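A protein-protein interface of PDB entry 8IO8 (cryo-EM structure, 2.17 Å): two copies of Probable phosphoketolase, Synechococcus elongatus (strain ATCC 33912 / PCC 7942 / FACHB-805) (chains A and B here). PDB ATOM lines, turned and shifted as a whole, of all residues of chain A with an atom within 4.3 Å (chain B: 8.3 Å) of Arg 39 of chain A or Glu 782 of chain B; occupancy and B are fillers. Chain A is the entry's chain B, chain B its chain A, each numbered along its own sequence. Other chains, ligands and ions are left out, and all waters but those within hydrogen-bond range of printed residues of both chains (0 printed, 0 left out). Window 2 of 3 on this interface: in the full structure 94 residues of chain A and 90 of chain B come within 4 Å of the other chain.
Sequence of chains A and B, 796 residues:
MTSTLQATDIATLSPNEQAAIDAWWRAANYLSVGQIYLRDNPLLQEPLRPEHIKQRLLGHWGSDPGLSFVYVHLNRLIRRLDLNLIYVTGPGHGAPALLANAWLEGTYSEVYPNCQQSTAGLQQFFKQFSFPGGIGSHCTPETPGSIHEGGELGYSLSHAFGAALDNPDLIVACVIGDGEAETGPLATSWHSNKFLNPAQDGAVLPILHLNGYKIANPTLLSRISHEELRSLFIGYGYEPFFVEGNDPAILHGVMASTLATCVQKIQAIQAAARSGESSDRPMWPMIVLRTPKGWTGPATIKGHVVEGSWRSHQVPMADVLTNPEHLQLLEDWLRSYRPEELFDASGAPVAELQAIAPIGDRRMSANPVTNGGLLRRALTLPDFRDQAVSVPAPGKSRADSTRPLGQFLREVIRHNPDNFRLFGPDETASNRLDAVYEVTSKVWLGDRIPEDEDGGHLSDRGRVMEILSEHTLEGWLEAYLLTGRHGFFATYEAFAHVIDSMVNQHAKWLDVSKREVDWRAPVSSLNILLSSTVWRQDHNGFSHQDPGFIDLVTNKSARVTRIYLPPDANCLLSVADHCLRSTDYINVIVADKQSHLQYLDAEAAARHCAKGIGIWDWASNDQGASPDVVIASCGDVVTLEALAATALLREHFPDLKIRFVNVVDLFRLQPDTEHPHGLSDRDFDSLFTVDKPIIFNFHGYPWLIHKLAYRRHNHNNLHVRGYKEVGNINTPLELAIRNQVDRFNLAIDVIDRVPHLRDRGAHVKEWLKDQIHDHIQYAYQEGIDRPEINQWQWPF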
ATOM      1  N   TYR A  37     -35.127  -2.740   6.652  1.00  0.00           N
ATOM      2  CA  TYR A  37     -34.470  -1.679   5.899  1.00  0.00           C
ATOM      3  C   TYR A  37     -34.851  -0.274   6.347  1.00  0.00           C
ATOM      4  O   TYR A  37     -33.971   0.557   6.576  1.00  0.00           O
ATOM      5  CB  TYR A  37     -34.775  -1.838   4.409  1.00  0.00           C
ATOM      6  CG  TYR A  37     -34.021  -2.961   3.754  1.00  0.00           C
ATOM      7  CD1 TYR A  37     -32.724  -2.777   3.309  1.00  0.00           C
ATOM      8  CD2 TYR A  37     -34.602  -4.204   3.580  1.00  0.00           C
ATOM      9  CE1 TYR A  37     -32.028  -3.798   2.709  1.00  0.00           C
ATOM     10  CE2 TYR A  37     -33.915  -5.232   2.982  1.00  0.00           C
ATOM     11  CZ  TYR A  37     -32.627  -5.023   2.548  1.00  0.00           C
ATOM     12  OH  TYR A  37     -31.932  -6.043   1.947  1.00  0.00           O
ATOM     13  N   LEU A  38     -36.140   0.019   6.457  1.00  0.00           N
ATOM     14  CA  LEU A  38     -36.586   1.395   6.617  1.00  0.00           C
ATOM     15  C   LEU A  38     -36.504   1.849   8.066  1.00  0.00           C
ATOM     16  O   LEU A  38     -36.769   1.080   8.991  1.00  0.00           O
ATOM     17  CB  LEU A  38     -38.016   1.553   6.114  1.00  0.00           C
ATOM     18  CG  LEU A  38     -38.271   1.134   4.673  1.00  0.00           C
ATOM     19  CD1 LEU A  38     -39.693   1.461   4.281  1.00  0.00           C
ATOM     20  CD2 LEU A  38     -37.290   1.811   3.747  1.00  0.00           C
ATOM     21  N   ARG A  39     -36.127   3.109   8.253  1.00  0.00           N
ATOM     22  CA  ARG A  39     -36.271   3.788   9.529  1.00  0.00           C
ATOM     23  C   ARG A  39     -37.173   5.004   9.425  1.00  0.00           C
ATOM     24  O   ARG A  39     -37.406   5.676  10.433  1.00  0.00           O
ATOM     25  CB  ARG A  39     -34.905   4.210  10.081  1.00  0.00           C
ATOM     26  CG  ARG A  39     -34.236   5.312   9.300  1.00  0.00           C
ATOM     27  CD  ARG A  39     -32.973   5.757   9.997  1.00  0.00           C
ATOM     28  NE  ARG A  39     -32.187   6.666   9.174  1.00  0.00           N
ATOM     29  CZ  ARG A  39     -31.025   7.186   9.538  1.00  0.00           C
ATOM     30  NH1 ARG A  39     -30.488   6.919  10.717  1.00  0.00           N
ATOM     31  NH2 ARG A  39     -30.384   7.993   8.700  1.00  0.00           N
ATOM     32  N   ASP A  40     -37.676   5.306   8.234  1.00  0.00           N
ATOM     33  CA  ASP A  40     -38.578   6.422   8.016  1.00  0.00           C
ATOM     34  C   ASP A  40     -39.345   6.143   6.737  1.00  0.00           C
ATOM     35  O   ASP A  40     -38.982   5.254   5.964  1.00  0.00           O
ATOM     36  CB  ASP A  40     -37.822   7.750   7.924  1.00  0.00           C
ATOM     37  CG  ASP A  40     -38.717   8.948   8.155  1.00  0.00           C
ATOM     38  OD1 ASP A  40     -39.949   8.813   8.002  1.00  0.00           O
ATOM     39  OD2 ASP A  40     -38.190  10.028   8.486  1.00  0.00           O
ATOM     40  N   GLU A  51     -31.692   8.660   3.308  1.00  0.00           N
ATOM     41  CA  GLU A  51     -31.899   9.004   4.709  1.00  0.00           C
ATOM     42  C   GLU A  51     -33.025   8.199   5.344  1.00  0.00           C
ATOM     43  O   GLU A  51     -33.131   8.175   6.573  1.00  0.00           O
ATOM     44  CB  GLU A  51     -32.181  10.499   4.859  1.00  0.00           C
ATOM     45  CG  GLU A  51     -33.115  11.083   3.818  1.00  0.00           C
ATOM     46  CD  GLU A  51     -32.373  11.625   2.609  1.00  0.00           C
ATOM     47  OE1 GLU A  51     -31.206  11.234   2.398  1.00  0.00           O
ATOM     48  OE2 GLU A  51     -32.957  12.448   1.873  1.00  0.00           O
ATOM     49  N   HIS A  52     -33.865   7.546   4.541  1.00  0.00           N
ATOM     50  CA  HIS A  52     -34.903   6.675   5.070  1.00  0.00           C
ATOM     51  C   HIS A  52     -34.393   5.287   5.416  1.00  0.00           C
ATOM     52  O   HIS A  52     -35.090   4.546   6.113  1.00  0.00           O
ATOM     53  CB  HIS A  52     -36.045   6.540   4.066  1.00  0.00           C
ATOM     54  CG  HIS A  52     -36.696   7.837   3.711  1.00  0.00           C
ATOM     55  ND1 HIS A  52     -36.701   8.923   4.557  1.00  0.00           N
ATOM     56  CD2 HIS A  52     -37.362   8.224   2.598  1.00  0.00           C
ATOM     57  CE1 HIS A  52     -37.345   9.923   3.982  1.00  0.00           C
ATOM     58  NE2 HIS A  52     -37.754   9.524   2.792  1.00  0.00           N
ATOM     59  N   ILE A  53     -33.211   4.928   4.962  1.00  0.00           N
ATOM     60  CA  ILE A  53     -32.698   3.571   5.091  1.00  0.00           C
ATOM     61  C   ILE A  53     -31.896   3.456   6.375  1.00  0.00           C
ATOM     62  O   ILE A  53     -31.168   4.377   6.756  1.00  0.00           O
ATOM     63  CB  ILE A  53     -31.842   3.199   3.867  1.00  0.00           C
ATOM     64  CG1 ILE A  53     -32.623   3.455   2.585  1.00  0.00           C
ATOM     65  CG2 ILE A  53     -31.412   1.753   3.935  1.00  0.00           C
ATOM     66  CD1 ILE A  53     -33.910   2.696   2.508  1.00  0.00           C
ATOM     67  N   LYS A  54     -32.037   2.322   7.050  1.00  0.00           N
ATOM     68  CA  LYS A  54     -31.230   2.051   8.227  1.00  0.00           C
ATOM     69  C   LYS A  54     -29.766   1.889   7.854  1.00  0.00           C
ATOM     70  O   LYS A  54     -29.422   1.437   6.760  1.00  0.00           O
ATOM     71  CB  LYS A  54     -31.702   0.784   8.928  1.00  0.00           C
ATOM     72  CG  LYS A  54     -33.005   0.911   9.662  1.00  0.00           C
ATOM     73  CD  LYS A  54     -33.312  -0.385  10.364  1.00  0.00           C
ATOM     74  CE  LYS A  54     -34.636  -0.323  11.066  1.00  0.00           C
ATOM     75  NZ  LYS A  54     -34.972  -1.635  11.661  1.00  0.00           N
ATOM     76  N   GLN A  55     -28.901   2.260   8.785  1.00  0.00           N
ATOM     77  CA  GLN A  55     -27.487   1.945   8.715  1.00  0.00           C
ATOM     78  C   GLN A  55     -27.207   0.758   9.626  1.00  0.00           C
ATOM     79  O   GLN A  55     -27.833   0.606  10.677  1.00  0.00           O
ATOM     80  CB  GLN A  55     -26.648   3.153   9.121  1.00  0.00           C
ATOM     81  CG  GLN A  55     -26.956   4.385   8.294  1.00  0.00           C
ATOM     82  CD  GLN A  55     -26.418   5.655   8.906  1.00  0.00           C
ATOM     83  OE1 GLN A  55     -26.554   5.884  10.106  1.00  0.00           O
ATOM     84  NE2 GLN A  55     -25.801   6.492   8.083  1.00  0.00           N
ATOM     85  N   LYS A 127     -38.594   1.556  12.734  1.00  0.00           N
ATOM     86  CA  LYS A 127     -37.362   2.120  13.274  1.00  0.00           C
ATOM     87  C   LYS A 127     -36.784   1.251  14.384  1.00  0.00           C
ATOM     88  O   LYS A 127     -35.563   1.112  14.499  1.00  0.00           O
ATOM     89  CB  LYS A 127     -37.638   3.536  13.776  1.00  0.00           C
ATOM     90  CG  LYS A 127     -36.570   4.151  14.648  1.00  0.00           C
ATOM     91  CD  LYS A 127     -35.352   4.544  13.851  1.00  0.00           C
ATOM     92  CE  LYS A 127     -34.655   5.725  14.497  1.00  0.00           C
ATOM     93  NZ  LYS A 127     -34.535   5.546  15.969  1.00  0.00           N
ATOM     94  N   PHE A 131     -32.240  -2.094  16.277  1.00  0.00           N
ATOM     95  CA  PHE A 131     -31.762  -0.735  16.439  1.00  0.00           C
ATOM     96  C   PHE A 131     -31.362  -0.507  17.887  1.00  0.00           C
ATOM     97  O   PHE A 131     -31.984  -1.060  18.799  1.00  0.00           O
ATOM     98  CB  PHE A 131     -32.851   0.265  16.039  1.00  0.00           C
ATOM     99  CG  PHE A 131     -32.327   1.579  15.565  1.00  0.00           C
ATOM    100  CD1 PHE A 131     -31.920   1.740  14.255  1.00  0.00           C
ATOM    101  CD2 PHE A 131     -32.258   2.660  16.419  1.00  0.00           C
ATOM    102  CE1 PHE A 131     -31.445   2.949  13.812  1.00  0.00           C
ATOM    103  CE2 PHE A 131     -31.782   3.871  15.980  1.00  0.00           C
ATOM    104  CZ  PHE A 131     -31.377   4.016  14.675  1.00  0.00           C
ATOM    105  N   THR B 731     -24.239  -0.702  19.245  1.00  0.00           N
ATOM    106  CA  THR B 731     -23.161  -0.404  18.322  1.00  0.00           C
ATOM    107  C   THR B 731     -21.837  -0.822  18.957  1.00  0.00           C
ATOM    108  O   THR B 731     -21.744  -0.955  20.179  1.00  0.00           O
ATOM    109  CB  THR B 731     -23.147   1.085  17.977  1.00  0.00           C
ATOM    110  OG1 THR B 731     -22.683   1.832  19.105  1.00  0.00           O
ATOM    111  CG2 THR B 731     -24.536   1.561  17.603  1.00  0.00           C
ATOM    112  N   HIS B 775     -21.463  10.158  22.446  1.00  0.00           N
ATOM    113  CA  HIS B 775     -21.444   9.004  21.556  1.00  0.00           C
ATOM    114  C   HIS B 775     -22.635   8.088  21.789  1.00  0.00           C
ATOM    115  O   HIS B 775     -23.137   7.482  20.839  1.00  0.00           O
ATOM    116  CB  HIS B 775     -20.132   8.243  21.717  1.00  0.00           C
ATOM    117  CG  HIS B 775     -18.942   8.988  21.200  1.00  0.00           C
ATOM    118  ND1 HIS B 775     -18.749   9.238  19.861  1.00  0.00           N
ATOM    119  CD2 HIS B 775     -17.889   9.541  21.842  1.00  0.00           C
ATOM    120  CE1 HIS B 775     -17.627   9.914  19.698  1.00  0.00           C
ATOM    121  NE2 HIS B 775     -17.086  10.112  20.886  1.00  0.00           N
ATOM    122  N   ILE B 776     -23.094   7.966  23.034  1.00  0.00           N
ATOM    123  CA  ILE B 776     -24.289   7.172  23.305  1.00  0.00           C
ATOM    124  C   ILE B 776     -25.510   7.803  22.648  1.00  0.00           C
ATOM    125  O   ILE B 776     -26.341   7.106  22.056  1.00  0.00           O
ATOM    126  CB  ILE B 776     -24.486   6.999  24.820  1.00  0.00           C
ATOM    127  CG1 ILE B 776     -23.391   6.114  25.408  1.00  0.00           C
ATOM    128  CG2 ILE B 776     -25.845   6.402  25.119  1.00  0.00           C
ATOM    129  CD1 ILE B 776     -23.413   4.700  24.899  1.00  0.00           C
ATOM    130  N   GLN B 777     -25.642   9.128  22.742  1.00  0.00           N
ATOM    131  CA  GLN B 777     -26.783   9.803  22.133  1.00  0.00           C
ATOM    132  C   GLN B 777     -26.759   9.679  20.617  1.00  0.00           C
ATOM    133  O   GLN B 777     -27.803   9.484  19.988  1.00  0.00           O
ATOM    134  CB  GLN B 777     -26.810  11.271  22.546  1.00  0.00           C
ATOM    135  CG  GLN B 777     -27.070  11.482  24.020  1.00  0.00           C
ATOM    136  CD  GLN B 777     -28.307  10.755  24.494  1.00  0.00           C
ATOM    137  OE1 GLN B 777     -28.235   9.883  25.359  1.00  0.00           O
ATOM    138  NE2 GLN B 777     -29.454  11.109  23.929  1.00  0.00           N
ATOM    139  N   TYR B 778     -25.578   9.801  20.011  1.00  0.00           N
ATOM    140  CA  TYR B 778     -25.480   9.664  18.563  1.00  0.00           C
ATOM    141  C   TYR B 778     -25.822   8.248  18.121  1.00  0.00           C
ATOM    142  O   TYR B 778     -26.416   8.050  17.057  1.00  0.00           O
ATOM    143  CB  TYR B 778     -24.083  10.050  18.094  1.00  0.00           C
ATOM    144  CG  TYR B 778     -23.928  10.066  16.595  1.00  0.00           C
ATOM    145  CD1 TYR B 778     -24.250  11.194  15.860  1.00  0.00           C
ATOM    146  CD2 TYR B 778     -23.457   8.953  15.914  1.00  0.00           C
ATOM    147  CE1 TYR B 778     -24.108  11.215  14.493  1.00  0.00           C
ATOM    148  CE2 TYR B 778     -23.313   8.965  14.548  1.00  0.00           C
ATOM    149  CZ  TYR B 778     -23.640  10.100  13.841  1.00  0.00           C
ATOM    150  OH  TYR B 778     -23.499  10.119  12.475  1.00  0.00           O
ATOM    151  N   ALA B 779     -25.448   7.250  18.921  1.00  0.00           N
ATOM    152  CA  ALA B 779     -25.775   5.872  18.582  1.00  0.00           C
ATOM    153  C   ALA B 779     -27.274   5.622  18.628  1.00  0.00           C
ATOM    154  O   ALA B 779     -27.785   4.799  17.863  1.00  0.00           O
ATOM    155  CB  ALA B 779     -25.052   4.912  19.523  1.00  0.00           C
ATOM    156  N   TYR B 780     -27.994   6.313  19.512  1.00  0.00           N
ATOM    157  CA  TYR B 780     -29.435   6.111  19.595  1.00  0.00           C
ATOM    158  C   TYR B 780     -30.170   6.764  18.434  1.00  0.00           C
ATOM    159  O   TYR B 780     -31.191   6.239  17.981  1.00  0.00           O
ATOM    160  CB  TYR B 780     -29.967   6.638  20.923  1.00  0.00           C
ATOM    161  CG  TYR B 780     -29.766   5.681  22.068  1.00  0.00           C
ATOM    162  CD1 TYR B 780     -29.525   4.337  21.833  1.00  0.00           C
ATOM    163  CD2 TYR B 780     -29.818   6.116  23.381  1.00  0.00           C
ATOM    164  CE1 TYR B 780     -29.341   3.455  22.871  1.00  0.00           C
ATOM    165  CE2 TYR B 780     -29.635   5.240  24.427  1.00  0.00           C
ATOM    166  CZ  TYR B 780     -29.396   3.910  24.165  1.00  0.00           C
ATOM    167  OH  TYR B 780     -29.213   3.027  25.201  1.00  0.00           O
ATOM    168  N   GLN B 781     -29.683   7.900  17.945  1.00  0.00           N
ATOM    169  CA  GLN B 781     -30.367   8.601  16.870  1.00  0.00           C
ATOM    170  C   GLN B 781     -29.920   8.167  15.483  1.00  0.00           C
ATOM    171  O   GLN B 781     -30.538   8.579  14.498  1.00  0.00           O
ATOM    172  CB  GLN B 781     -30.167  10.112  17.009  1.00  0.00           C
ATOM    173  CG  GLN B 781     -28.737  10.570  16.820  1.00  0.00           C
ATOM    174  CD  GLN B 781     -28.603  12.079  16.856  1.00  0.00           C
ATOM    175  OE1 GLN B 781     -29.578  12.803  16.658  1.00  0.00           O
ATOM    176  NE2 GLN B 781     -27.394  12.561  17.114  1.00  0.00           N
ATOM    177  N   GLU B 782     -28.875   7.350  15.375  1.00  0.00           N
ATOM    178  CA  GLU B 782     -28.361   6.961  14.069  1.00  0.00           C
ATOM    179  C   GLU B 782     -28.237   5.451  13.940  1.00  0.00           C
ATOM    180  O   GLU B 782     -28.312   4.909  12.835  1.00  0.00           O
ATOM    181  CB  GLU B 782     -27.003   7.615  13.811  1.00  0.00           C
ATOM    182  CG  GLU B 782     -27.039   9.126  13.778  1.00  0.00           C
ATOM    183  CD  GLU B 782     -27.909   9.659  12.660  1.00  0.00           C
ATOM    184  OE1 GLU B 782     -27.955   9.024  11.587  1.00  0.00           O
ATOM    185  OE2 GLU B 782     -28.551  10.710  12.855  1.00  0.00           O
ATOM    186  N   GLY B 783     -28.038   4.764  15.059  1.00  0.00           N
ATOM    187  CA  GLY B 783     -27.787   3.343  15.027  1.00  0.00           C
ATOM    188  C   GLY B 783     -26.372   2.969  14.663  1.00  0.00           C
ATOM    189  O   GLY B 783     -26.064   1.774  14.581  1.00  0.00           O
ATOM    190  N   ILE B 784     -25.502   3.952  14.439  1.00  0.00           N
ATOM    191  CA  ILE B 784     -24.120   3.723  14.049  1.00  0.00           C
ATOM    192  C   ILE B 784     -23.244   4.687  14.838  1.00  0.00           C
ATOM    193  O   ILE B 784     -23.716   5.687  15.380  1.00  0.00           O
ATOM    194  CB  ILE B 784     -23.918   3.908  12.527  1.00  0.00           C
ATOM    195  CG1 ILE B 784     -22.733   3.085  12.029  1.00  0.00           C
ATOM    196  CG2 ILE B 784     -23.744   5.375  12.178  1.00  0.00           C
ATOM    197  CD1 ILE B 784     -22.955   1.597  12.123  1.00  0.00           C
ATOM    198  N   ASP B 785     -21.958   4.365  14.915  1.00  0.00           N
ATOM    199  CA  ASP B 785     -21.007   5.255  15.559  1.00  0.00           C
ATOM    200  C   ASP B 785     -20.570   6.356  14.599  1.00  0.00           C
ATOM    201  O   ASP B 785     -20.770   6.275  13.385  1.00  0.00           O
ATOM    202  CB  ASP B 785     -19.790   4.478  16.054  1.00  0.00           C
ATOM    203  CG  ASP B 785     -20.153   3.414  17.070  1.00  0.00           C
ATOM    204  OD1 ASP B 785     -21.033   3.674  17.917  1.00  0.00           O
ATOM    205  OD2 ASP B 785     -19.560   2.316  17.021  1.00  0.00           O
ATOM    206  N   ARG B 786     -19.963   7.396  15.160  1.00  0.00           N
ATOM    207  CA  ARG B 786     -19.487   8.502  14.351  1.00  0.00           C
ATOM    208  C   ARG B 786     -18.328   8.055  13.462  1.00  0.00           C
ATOM    209  O   ARG B 786     -17.597   7.122  13.804  1.00  0.00           O
ATOM    210  CB  ARG B 786     -19.040   9.660  15.235  1.00  0.00           C
ATOM    211  CG  ARG B 786     -20.172  10.379  15.928  1.00  0.00           C
ATOM    212  CD  ARG B 786     -19.668  11.597  16.667  1.00  0.00           C
ATOM    213  NE  ARG B 786     -20.755  12.339  17.289  1.00  0.00           N
ATOM    214  CZ  ARG B 786     -21.477  13.262  16.671  1.00  0.00           C
ATOM    215  NH1 ARG B 786     -21.254  13.583  15.407  1.00  0.00           N
ATOM    216  NH2 ARG B 786     -22.450  13.878  17.335  1.00  0.00           N
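NH1 of Arg 39 of chain A is in salt-bridge range of OE1 of Glu 782 of chain B (3.4 Å).
The side-chain amide oxygen (OE1) of Gln 55 of chain A lies close to the backbone carbonyl oxygen (O) of Glu 782 of chain B, 3.4 Å away.
The guanidinium group (NE) of Arg 39 of chain A lies within hydrogen-bond range of the backbone carbonyl oxygen (O) of Glu 51 of chain A.
The backbone NH of Arg 39 of chain A lies within hydrogen-bond range of the backbone carbonyl oxygen of His 52 of chain A.
The guanidinium group of Arg 39 of chain A sits at hydrogen-bond distance from the backbone carbonyl oxygen of Ile 53 of chain A.
Among the printed residues, merely in contact across the chains: Phe 131 of chain A with Tyr 780 of chain B, Phe 131 of chain A with Gly 783 of chain B, Gln 55 of chain A with Ile 784 of chain B, Phe 131 of chain A with Glu 782 of chain B and Lys 127 of chain A with Tyr 780 of chain B.
Arg 39 of chain A touches one residue of chain B.
Of the printed residues of chain B, Gln 55 of chain A touches Glu 782 and Ile 784.
Of the printed residues of chain B, Lys 127 of chain A touches Tyr 780 (3.96 Å).
Of the printed residues of chain B, Phe 131 of chain A touches Tyr 780 (3.2 Å), Glu 782 (3.5 Å) and Gly 783 (3.4 Å).
Tyr 778 of chain B touches none of the printed residues of chain A.
Ala 779 of chain B touches none of the printed residues of chain A.
Of chain A, only Arg 39, Gln 55 and Phe 131 come within 4 Å of Glu 782 of chain B.
Of the printed residues of chain A, Gly 783 of chain B touches Phe 131 (3.4 Å).
Of the printed residues of chain A, Ile 784 of chain B touches Gln 55.
The nearest residue of chain B that does not touch Arg 39 of chain A is Gln 781 of chain B (4.1 Å).
The nearest printed residue of chain A that does not touch Glu 782 of chain B is Lys 127 of chain A (6.0 Å).
The nearest printed residue of chain A that does not touch Gly 783 of chain B is Gln 55 of chain A (4.4 Å).
Hydrophobic or aromatic side chains of chain B that line the printed part of chain A: Ile 784.
Hydrophobic or aromatic side chains of chain A that line the printed part of chain B: Phe 131.
No position is printed for both chains.
Of the 7 pairs that touch across the chains among the printed residues, none has its exchanged pair printed and touching as well.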
